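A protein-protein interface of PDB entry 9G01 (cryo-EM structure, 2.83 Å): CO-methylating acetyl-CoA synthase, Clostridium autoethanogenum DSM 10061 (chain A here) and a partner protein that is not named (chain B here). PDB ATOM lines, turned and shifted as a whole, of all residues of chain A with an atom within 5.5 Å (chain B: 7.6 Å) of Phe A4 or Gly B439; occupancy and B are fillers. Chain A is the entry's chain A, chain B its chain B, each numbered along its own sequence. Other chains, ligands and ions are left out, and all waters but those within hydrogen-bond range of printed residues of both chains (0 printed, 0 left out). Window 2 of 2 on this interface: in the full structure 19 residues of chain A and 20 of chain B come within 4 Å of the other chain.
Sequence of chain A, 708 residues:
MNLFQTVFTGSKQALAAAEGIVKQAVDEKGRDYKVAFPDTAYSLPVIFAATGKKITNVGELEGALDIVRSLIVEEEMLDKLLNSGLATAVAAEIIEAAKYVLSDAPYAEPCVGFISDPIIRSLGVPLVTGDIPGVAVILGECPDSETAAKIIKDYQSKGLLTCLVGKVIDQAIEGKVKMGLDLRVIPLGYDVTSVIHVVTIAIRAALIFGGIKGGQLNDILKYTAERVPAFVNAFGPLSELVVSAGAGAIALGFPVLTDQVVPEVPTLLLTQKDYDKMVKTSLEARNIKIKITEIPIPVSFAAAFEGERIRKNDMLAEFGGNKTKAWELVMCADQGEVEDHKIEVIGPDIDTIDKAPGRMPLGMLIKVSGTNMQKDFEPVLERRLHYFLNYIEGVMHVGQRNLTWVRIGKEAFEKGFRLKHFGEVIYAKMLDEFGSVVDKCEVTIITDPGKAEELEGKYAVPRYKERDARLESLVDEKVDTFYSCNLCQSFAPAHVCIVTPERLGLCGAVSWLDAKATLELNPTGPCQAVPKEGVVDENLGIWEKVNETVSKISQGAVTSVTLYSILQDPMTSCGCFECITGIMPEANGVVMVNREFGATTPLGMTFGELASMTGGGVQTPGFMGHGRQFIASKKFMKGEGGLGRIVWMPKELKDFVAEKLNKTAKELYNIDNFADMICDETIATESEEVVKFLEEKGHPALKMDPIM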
ATOM      1  N   ASN A   2      -5.333  33.918 -20.537  1.00  0.00           N
ATOM      2  CA  ASN A   2      -6.175  33.015 -21.299  1.00  0.00           C
ATOM      3  C   ASN A   2      -7.624  33.129 -20.815  1.00  0.00           C
ATOM      4  O   ASN A   2      -7.944  33.890 -19.896  1.00  0.00           O
ATOM      5  CB  ASN A   2      -5.621  31.588 -21.221  1.00  0.00           C
ATOM      6  CG  ASN A   2      -5.562  31.041 -19.792  1.00  0.00           C
ATOM      7  OD1 ASN A   2      -6.490  31.223 -19.015  1.00  0.00           O
ATOM      8  ND2 ASN A   2      -4.463  30.369 -19.448  1.00  0.00           N
ATOM      9  N   LEU A   3      -8.508  32.321 -21.406  1.00  0.00           N
ATOM     10  CA  LEU A   3      -9.934  32.397 -21.097  1.00  0.00           C
ATOM     11  C   LEU A   3     -10.214  32.088 -19.632  1.00  0.00           C
ATOM     12  O   LEU A   3     -10.945  32.827 -18.959  1.00  0.00           O
ATOM     13  CB  LEU A   3     -10.713  31.436 -22.003  1.00  0.00           C
ATOM     14  CG  LEU A   3     -12.235  31.422 -21.777  1.00  0.00           C
ATOM     15  CD1 LEU A   3     -12.850  32.798 -22.085  1.00  0.00           C
ATOM     16  CD2 LEU A   3     -12.898  30.322 -22.618  1.00  0.00           C
ATOM     17  N   PHE A   4      -9.613  31.019 -19.108  1.00  0.00           N
ATOM     18  CA  PHE A   4      -9.839  30.635 -17.719  1.00  0.00           C
ATOM     19  C   PHE A   4      -9.385  31.732 -16.772  1.00  0.00           C
ATOM     20  O   PHE A   4     -10.085  32.065 -15.806  1.00  0.00           O
ATOM     21  CB  PHE A   4      -9.108  29.333 -17.390  1.00  0.00           C
ATOM     22  CG  PHE A   4      -9.786  28.096 -17.909  1.00  0.00           C
ATOM     23  CD1 PHE A   4      -9.601  27.694 -19.234  1.00  0.00           C
ATOM     24  CD2 PHE A   4     -10.611  27.330 -17.076  1.00  0.00           C
ATOM     25  CE1 PHE A   4     -10.228  26.544 -19.739  1.00  0.00           C
ATOM     26  CE2 PHE A   4     -11.244  26.177 -17.555  1.00  0.00           C
ATOM     27  CZ  PHE A   4     -11.055  25.777 -18.896  1.00  0.00           C
ATOM     28  N   GLN A   5      -8.205  32.291 -17.022  1.00  0.00           N
ATOM     29  CA  GLN A   5      -7.690  33.342 -16.157  1.00  0.00           C
ATOM     30  C   GLN A   5      -8.538  34.600 -16.266  1.00  0.00           C
ATOM     31  O   GLN A   5      -8.778  35.277 -15.263  1.00  0.00           O
ATOM     32  CB  GLN A   5      -6.226  33.638 -16.502  1.00  0.00           C
ATOM     33  CG  GLN A   5      -5.278  32.473 -16.161  1.00  0.00           C
ATOM     34  CD  GLN A   5      -5.460  31.999 -14.716  1.00  0.00           C
ATOM     35  OE1 GLN A   5      -5.623  30.808 -14.461  1.00  0.00           O
ATOM     36  NE2 GLN A   5      -5.460  32.944 -13.767  1.00  0.00           N
ATOM     37  N   THR A   6      -9.020  34.920 -17.468  1.00  0.00           N
ATOM     38  CA  THR A   6      -9.913  36.067 -17.610  1.00  0.00           C
ATOM     39  C   THR A   6     -11.192  35.877 -16.797  1.00  0.00           C
ATOM     40  O   THR A   6     -11.622  36.792 -16.083  1.00  0.00           O
ATOM     41  CB  THR A   6     -10.243  36.291 -19.089  1.00  0.00           C
ATOM     42  OG1 THR A   6      -9.035  36.391 -19.853  1.00  0.00           O
ATOM     43  CG2 THR A   6     -11.052  37.567 -19.279  1.00  0.00           C
ATOM     44  N   VAL A   7     -11.796  34.686 -16.865  1.00  0.00           N
ATOM     45  CA  VAL A   7     -13.027  34.422 -16.119  1.00  0.00           C
ATOM     46  C   VAL A   7     -12.776  34.476 -14.616  1.00  0.00           C
ATOM     47  O   VAL A   7     -13.570  35.051 -13.861  1.00  0.00           O
ATOM     48  CB  VAL A   7     -13.633  33.069 -16.544  1.00  0.00           C
ATOM     49  CG1 VAL A   7     -14.768  32.633 -15.595  1.00  0.00           C
ATOM     50  CG2 VAL A   7     -14.148  33.162 -17.981  1.00  0.00           C
ATOM     51  N   PHE A   8     -11.669  33.887 -14.158  1.00  0.00           N
ATOM     52  CA  PHE A   8     -11.350  33.920 -12.733  1.00  0.00           C
ATOM     53  C   PHE A   8     -11.120  35.350 -12.249  1.00  0.00           C
ATOM     54  O   PHE A   8     -11.620  35.741 -11.184  1.00  0.00           O
ATOM     55  CB  PHE A   8     -10.133  33.034 -12.443  1.00  0.00           C
ATOM     56  CG  PHE A   8     -10.375  31.548 -12.673  1.00  0.00           C
ATOM     57  CD1 PHE A   8     -11.648  30.983 -12.476  1.00  0.00           C
ATOM     58  CD2 PHE A   8      -9.328  30.718 -13.086  1.00  0.00           C
ATOM     59  CE1 PHE A   8     -11.882  29.600 -12.690  1.00  0.00           C
ATOM     60  CE2 PHE A   8      -9.531  29.334 -13.308  1.00  0.00           C
ATOM     61  CZ  PHE A   8     -10.818  28.771 -13.110  1.00  0.00           C
ATOM     62  N   THR A   9     -10.407  36.157 -13.037  1.00  0.00           N
ATOM     63  CA  THR A   9     -10.184  37.551 -12.665  1.00  0.00           C
ATOM     64  C   THR A   9     -11.498  38.314 -12.594  1.00  0.00           C
ATOM     65  O   THR A   9     -11.736  39.070 -11.642  1.00  0.00           O
ATOM     66  CB  THR A   9      -9.247  38.214 -13.684  1.00  0.00           C
ATOM     67  OG1 THR A   9      -7.969  37.567 -13.680  1.00  0.00           O
ATOM     68  CG2 THR A   9      -9.060  39.700 -13.384  1.00  0.00           C
ATOM     69  N   GLU A  75      -8.842  26.395 -11.013  1.00  0.00           N
ATOM     70  CA  GLU A  75      -8.225  25.274 -11.706  1.00  0.00           C
ATOM     71  C   GLU A  75      -8.762  25.243 -13.128  1.00  0.00           C
ATOM     72  O   GLU A  75      -9.975  25.347 -13.337  1.00  0.00           O
ATOM     73  CB  GLU A  75      -8.511  23.955 -10.979  1.00  0.00           C
ATOM     74  CG  GLU A  75      -7.749  23.855  -9.648  1.00  0.00           C
ATOM     75  CD  GLU A  75      -8.421  22.927  -8.647  1.00  0.00           C
ATOM     76  OE1 GLU A  75      -9.383  22.235  -9.029  1.00  0.00           O
ATOM     77  OE2 GLU A  75      -7.992  22.897  -7.475  1.00  0.00           O
ATOM     78  N   GLU A  76      -7.860  25.124 -14.104  1.00  0.00           N
ATOM     79  CA  GLU A  76      -8.221  25.294 -15.513  1.00  0.00           C
ATOM     80  C   GLU A  76      -8.872  24.018 -16.051  1.00  0.00           C
ATOM     81  O   GLU A  76      -8.301  23.255 -16.832  1.00  0.00           O
ATOM     82  CB  GLU A  76      -7.006  25.709 -16.329  1.00  0.00           C
ATOM     83  CG  GLU A  76      -6.425  27.049 -15.854  1.00  0.00           C
ATOM     84  CD  GLU A  76      -5.500  27.683 -16.876  1.00  0.00           C
ATOM     85  OE1 GLU A  76      -5.080  26.977 -17.810  1.00  0.00           O
ATOM     86  OE2 GLU A  76      -5.203  28.889 -16.751  1.00  0.00           O
ATOM     87  N   MET A  77     -10.114  23.797 -15.608  1.00  0.00           N
ATOM     88  CA  MET A  77     -10.984  22.761 -16.144  1.00  0.00           C
ATOM     89  C   MET A  77     -12.357  23.380 -16.360  1.00  0.00           C
ATOM     90  O   MET A  77     -12.754  24.312 -15.655  1.00  0.00           O
ATOM     91  CB  MET A  77     -11.103  21.530 -15.207  1.00  0.00           C
ATOM     92  CG  MET A  77      -9.762  20.872 -14.829  1.00  0.00           C
ATOM     93  SD  MET A  77      -9.013  19.916 -16.176  1.00  0.00           S
ATOM     94  CE  MET A  77      -9.854  18.338 -16.054  1.00  0.00           C
ATOM     95  N   LEU A  78     -13.101  22.822 -17.314  1.00  0.00           N
ATOM     96  CA  LEU A  78     -14.327  23.467 -17.779  1.00  0.00           C
ATOM     97  C   LEU A  78     -15.350  23.629 -16.658  1.00  0.00           C
ATOM     98  O   LEU A  78     -16.023  24.666 -16.566  1.00  0.00           O
ATOM     99  CB  LEU A  78     -14.921  22.672 -18.943  1.00  0.00           C
ATOM    100  CG  LEU A  78     -16.216  23.266 -19.524  1.00  0.00           C
ATOM    101  CD1 LEU A  78     -15.978  24.665 -20.118  1.00  0.00           C
ATOM    102  CD2 LEU A  78     -16.805  22.325 -20.572  1.00  0.00           C
ATOM    103  N   LEU A  81     -14.613  26.635 -14.630  1.00  0.00           N
ATOM    104  CA  LEU A  81     -14.957  27.848 -15.363  1.00  0.00           C
ATOM    105  C   LEU A  81     -16.456  28.126 -15.286  1.00  0.00           C
ATOM    106  O   LEU A  81     -16.876  29.275 -15.089  1.00  0.00           O
ATOM    107  CB  LEU A  81     -14.476  27.720 -16.813  1.00  0.00           C
ATOM    108  CG  LEU A  81     -14.685  28.925 -17.738  1.00  0.00           C
ATOM    109  CD1 LEU A  81     -13.574  28.982 -18.793  1.00  0.00           C
ATOM    110  CD2 LEU A  81     -16.060  28.874 -18.417  1.00  0.00           C
ATOM    111  N   ALA B 433      -8.750  23.514 -33.103  1.00  0.00           N
ATOM    112  CA  ALA B 433      -7.815  24.540 -32.660  1.00  0.00           C
ATOM    113  C   ALA B 433      -8.473  25.451 -31.632  1.00  0.00           C
ATOM    114  O   ALA B 433      -7.838  25.842 -30.649  1.00  0.00           O
ATOM    115  CB  ALA B 433      -7.297  25.344 -33.856  1.00  0.00           C
ATOM    116  N   ASP B 434      -9.754  25.777 -31.824  1.00  0.00           N
ATOM    117  CA  ASP B 434     -10.464  26.645 -30.888  1.00  0.00           C
ATOM    118  C   ASP B 434     -10.612  25.991 -29.522  1.00  0.00           C
ATOM    119  O   ASP B 434     -10.325  26.616 -28.496  1.00  0.00           O
ATOM    120  CB  ASP B 434     -11.852  27.002 -31.429  1.00  0.00           C
ATOM    121  CG  ASP B 434     -11.799  27.884 -32.658  1.00  0.00           C
ATOM    122  OD1 ASP B 434     -10.853  28.693 -32.761  1.00  0.00           O
ATOM    123  OD2 ASP B 434     -12.694  27.773 -33.520  1.00  0.00           O
ATOM    124  N   VAL B 435     -11.014  24.720 -29.486  1.00  0.00           N
ATOM    125  CA  VAL B 435     -11.194  24.064 -28.191  1.00  0.00           C
ATOM    126  C   VAL B 435      -9.849  23.904 -27.489  1.00  0.00           C
ATOM    127  O   VAL B 435      -9.765  24.041 -26.263  1.00  0.00           O
ATOM    128  CB  VAL B 435     -11.937  22.718 -28.321  1.00  0.00           C
ATOM    129  CG1 VAL B 435     -13.335  22.930 -28.922  1.00  0.00           C
ATOM    130  CG2 VAL B 435     -11.144  21.713 -29.139  1.00  0.00           C
ATOM    131  N   LEU B 436      -8.772  23.670 -28.248  1.00  0.00           N
ATOM    132  CA  LEU B 436      -7.445  23.576 -27.637  1.00  0.00           C
ATOM    133  C   LEU B 436      -6.976  24.929 -27.109  1.00  0.00           C
ATOM    134  O   LEU B 436      -6.434  25.009 -26.001  1.00  0.00           O
ATOM    135  CB  LEU B 436      -6.430  23.020 -28.641  1.00  0.00           C
ATOM    136  CG  LEU B 436      -6.584  21.522 -28.945  1.00  0.00           C
ATOM    137  CD1 LEU B 436      -5.637  21.116 -30.075  1.00  0.00           C
ATOM    138  CD2 LEU B 436      -6.353  20.641 -27.688  1.00  0.00           C
ATOM    139  N   VAL B 437      -7.180  26.001 -27.876  1.00  0.00           N
ATOM    140  CA  VAL B 437      -6.702  27.313 -27.450  1.00  0.00           C
ATOM    141  C   VAL B 437      -7.499  27.809 -26.250  1.00  0.00           C
ATOM    142  O   VAL B 437      -6.936  28.380 -25.310  1.00  0.00           O
ATOM    143  CB  VAL B 437      -6.772  28.304 -28.629  1.00  0.00           C
ATOM    144  CG1 VAL B 437      -6.691  29.767 -28.138  1.00  0.00           C
ATOM    145  CG2 VAL B 437      -5.655  28.002 -29.648  1.00  0.00           C
ATOM    146  N   SER B 438      -8.820  27.617 -26.259  1.00  0.00           N
ATOM    147  CA  SER B 438      -9.637  28.108 -25.153  1.00  0.00           C
ATOM    148  C   SER B 438      -9.347  27.372 -23.848  1.00  0.00           C
ATOM    149  O   SER B 438      -9.603  27.926 -22.776  1.00  0.00           O
ATOM    150  CB  SER B 438     -11.138  28.020 -25.497  1.00  0.00           C
ATOM    151  OG  SER B 438     -11.596  26.675 -25.500  1.00  0.00           O
ATOM    152  N   GLY B 439      -8.778  26.169 -23.903  1.00  0.00           N
ATOM    153  CA  GLY B 439      -8.538  25.403 -22.702  1.00  0.00           C
ATOM    154  C   GLY B 439      -9.652  24.450 -22.325  1.00  0.00           C
ATOM    155  O   GLY B 439      -9.528  23.756 -21.309  1.00  0.00           O
ATOM    156  N   VAL B 440     -10.731  24.386 -23.111  1.00  0.00           N
ATOM    157  CA  VAL B 440     -11.765  23.380 -22.874  1.00  0.00           C
ATOM    158  C   VAL B 440     -11.153  21.992 -22.994  1.00  0.00           C
ATOM    159  O   VAL B 440     -11.454  21.090 -22.204  1.00  0.00           O
ATOM    160  CB  VAL B 440     -12.955  23.583 -23.832  1.00  0.00           C
ATOM    161  CG1 VAL B 440     -13.971  22.436 -23.707  1.00  0.00           C
ATOM    162  CG2 VAL B 440     -13.648  24.934 -23.544  1.00  0.00           C
ATOM    163  N   LEU B 441     -10.293  21.796 -23.990  1.00  0.00           N
ATOM    164  CA  LEU B 441      -9.422  20.633 -24.066  1.00  0.00           C
ATOM    165  C   LEU B 441      -8.015  21.069 -23.664  1.00  0.00           C
ATOM    166  O   LEU B 441      -7.503  22.075 -24.165  1.00  0.00           O
ATOM    167  CB  LEU B 441      -9.415  20.011 -25.464  1.00  0.00           C
ATOM    168  CG  LEU B 441     -10.700  19.287 -25.896  1.00  0.00           C
ATOM    169  CD1 LEU B 441     -10.436  18.611 -27.250  1.00  0.00           C
ATOM    170  CD2 LEU B 441     -11.226  18.270 -24.861  1.00  0.00           C
ATOM    171  N   ARG B 442      -7.414  20.325 -22.735  1.00  0.00           N
ATOM    172  CA  ARG B 442      -6.065  20.641 -22.277  1.00  0.00           C
ATOM    173  C   ARG B 442      -5.025  20.299 -23.335  1.00  0.00           C
ATOM    174  O   ARG B 442      -3.996  20.978 -23.428  1.00  0.00           O
ATOM    175  CB  ARG B 442      -5.775  19.904 -20.965  1.00  0.00           C
ATOM    176  CG  ARG B 442      -6.889  20.080 -19.896  1.00  0.00           C
ATOM    177  CD  ARG B 442      -7.255  21.570 -19.668  1.00  0.00           C
ATOM    178  NE  ARG B 442      -6.094  22.318 -19.197  1.00  0.00           N
ATOM    179  CZ  ARG B 442      -5.955  23.637 -19.242  1.00  0.00           C
ATOM    180  NH1 ARG B 442      -6.886  24.417 -19.757  1.00  0.00           N
ATOM    181  NH2 ARG B 442      -4.845  24.189 -18.752  1.00  0.00           N
ATOM    182  N   GLY B 443      -5.281  19.281 -24.148  1.00  0.00           N
ATOM    183  CA  GLY B 443      -4.359  18.913 -25.202  1.00  0.00           C
ATOM    184  C   GLY B 443      -4.835  17.677 -25.934  1.00  0.00           C
ATOM    185  O   GLY B 443      -5.957  17.206 -25.744  1.00  0.00           O
ATOM    186  N   ASP B 472      -9.107  15.615 -19.460  1.00  0.00           N
ATOM    187  CA  ASP B 472      -9.540  16.427 -20.598  1.00  0.00           C
ATOM    188  C   ASP B 472      -8.442  16.525 -21.662  1.00  0.00           C
ATOM    189  O   ASP B 472      -8.228  17.575 -22.268  1.00  0.00           O
ATOM    190  CB  ASP B 472     -10.005  17.824 -20.167  1.00  0.00           C
ATOM    191  CG  ASP B 472     -11.414  17.810 -19.587  1.00  0.00           C
ATOM    192  OD1 ASP B 472     -12.160  16.863 -19.900  1.00  0.00           O
ATOM    193  OD2 ASP B 472     -11.780  18.729 -18.824  1.00  0.00           O
ATOM    194  N   GLY B 503     -14.555  18.837 -19.724  1.00  0.00           N
ATOM    195  CA  GLY B 503     -14.346  19.490 -21.008  1.00  0.00           C
ATOM    196  C   GLY B 503     -14.383  18.516 -22.171  1.00  0.00           C
ATOM    197  O   GLY B 503     -15.002  18.785 -23.205  1.00  0.00           O
ATOM    198  N   ARG B 625       1.409  25.138 -22.679  1.00  0.00           N
ATOM    199  CA  ARG B 625       0.312  26.096 -22.794  1.00  0.00           C
ATOM    200  C   ARG B 625       0.700  27.450 -22.217  1.00  0.00           C
ATOM    201  O   ARG B 625       0.415  28.495 -22.813  1.00  0.00           O
ATOM    202  CB  ARG B 625      -0.935  25.569 -22.084  1.00  0.00           C
ATOM    203  CG  ARG B 625      -1.569  24.336 -22.737  1.00  0.00           C
ATOM    204  CD  ARG B 625      -2.829  23.932 -21.968  1.00  0.00           C
ATOM    205  NE  ARG B 625      -3.840  24.976 -22.098  1.00  0.00           N
ATOM    206  CZ  ARG B 625      -4.705  25.063 -23.100  1.00  0.00           C
ATOM    207  NH1 ARG B 625      -4.809  24.109 -24.008  1.00  0.00           N
ATOM    208  NH2 ARG B 625      -5.477  26.143 -23.204  1.00  0.00           N
ATOM    209  N   ILE B 630      -1.892  30.307 -23.808  1.00  0.00           N
ATOM    210  CA  ILE B 630      -3.269  29.815 -23.760  1.00  0.00           C
ATOM    211  C   ILE B 630      -3.564  29.151 -22.416  1.00  0.00           C
ATOM    212  O   ILE B 630      -4.642  28.594 -22.209  1.00  0.00           O
ATOM    213  CB  ILE B 630      -3.541  28.836 -24.920  1.00  0.00           C
ATOM    214  CG1 ILE B 630      -2.618  27.605 -24.803  1.00  0.00           C
ATOM    215  CG2 ILE B 630      -3.372  29.564 -26.267  1.00  0.00           C
ATOM    216  CD1 ILE B 630      -2.864  26.544 -25.883  1.00  0.00           C
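Of the 13 printed residues of chain A, 6 touch a printed residue of chain B. Hydrophobic or aromatic side chains of chain A within 4 Å of the printed part of chain B: Leu A3, Phe A4, Met A77 and Leu A78. Among the printed residues, 8 pairs touch across the chains.
Leu A3 touches Ser B438 (CB to O, 3.8 Å). CE1 of Phe A4 touches O of Ser B438 (3.4 Å). Phe A4 touches Gly B439. Phe A4 touches Arg B442 (CE1 to NH1, 3.96 Å). Asp B472 touches Met A77. Leu A78 touches Gly B503 (CD2 to CA, 3.8 Å).
The backbone NH (N) of Gln A5 is in hydrogen-bond range of the side-chain amide oxygen (OD1) of Asn A2, at 2.8 Å. The side-chain hydroxyl of Thr A6 sits at hydrogen-bond distance from the backbone carbonyl oxygen of Asn A2 (2.7 Å). The side-chain amide oxygen (OE1) of Gln A5 sits close to the side-chain carboxylate (OE2) of Glu A76 (3.0 Å). O of Asp B434 sits at hydrogen-bond distance from OG of Ser B438, at 3.3 Å. OG of Ser B438 lies within hydrogen-bond range of O of Val B435, 3.3 Å away. NH2 of Arg B625 lies within hydrogen-bond range of O of Ile B630 (2.8 Å).
Gly B439 touches just one residue of chain A: Phe A4. Of the printed residues of chain A, Ile B630 touches Asn A2. Printed residues of chain B within 4 Å of Leu A78: Gly B503. The nearest printed residue of chain A that does not touch Ser B438 is Asn A2 (5.6 Å).
ND2 of Asn A2 lies within hydrogen-bond range of O of Ile B630 (3.3 Å). OE1 of Glu A76 is in salt-bridge range of NH2 of Arg B442, at 3.0 Å.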
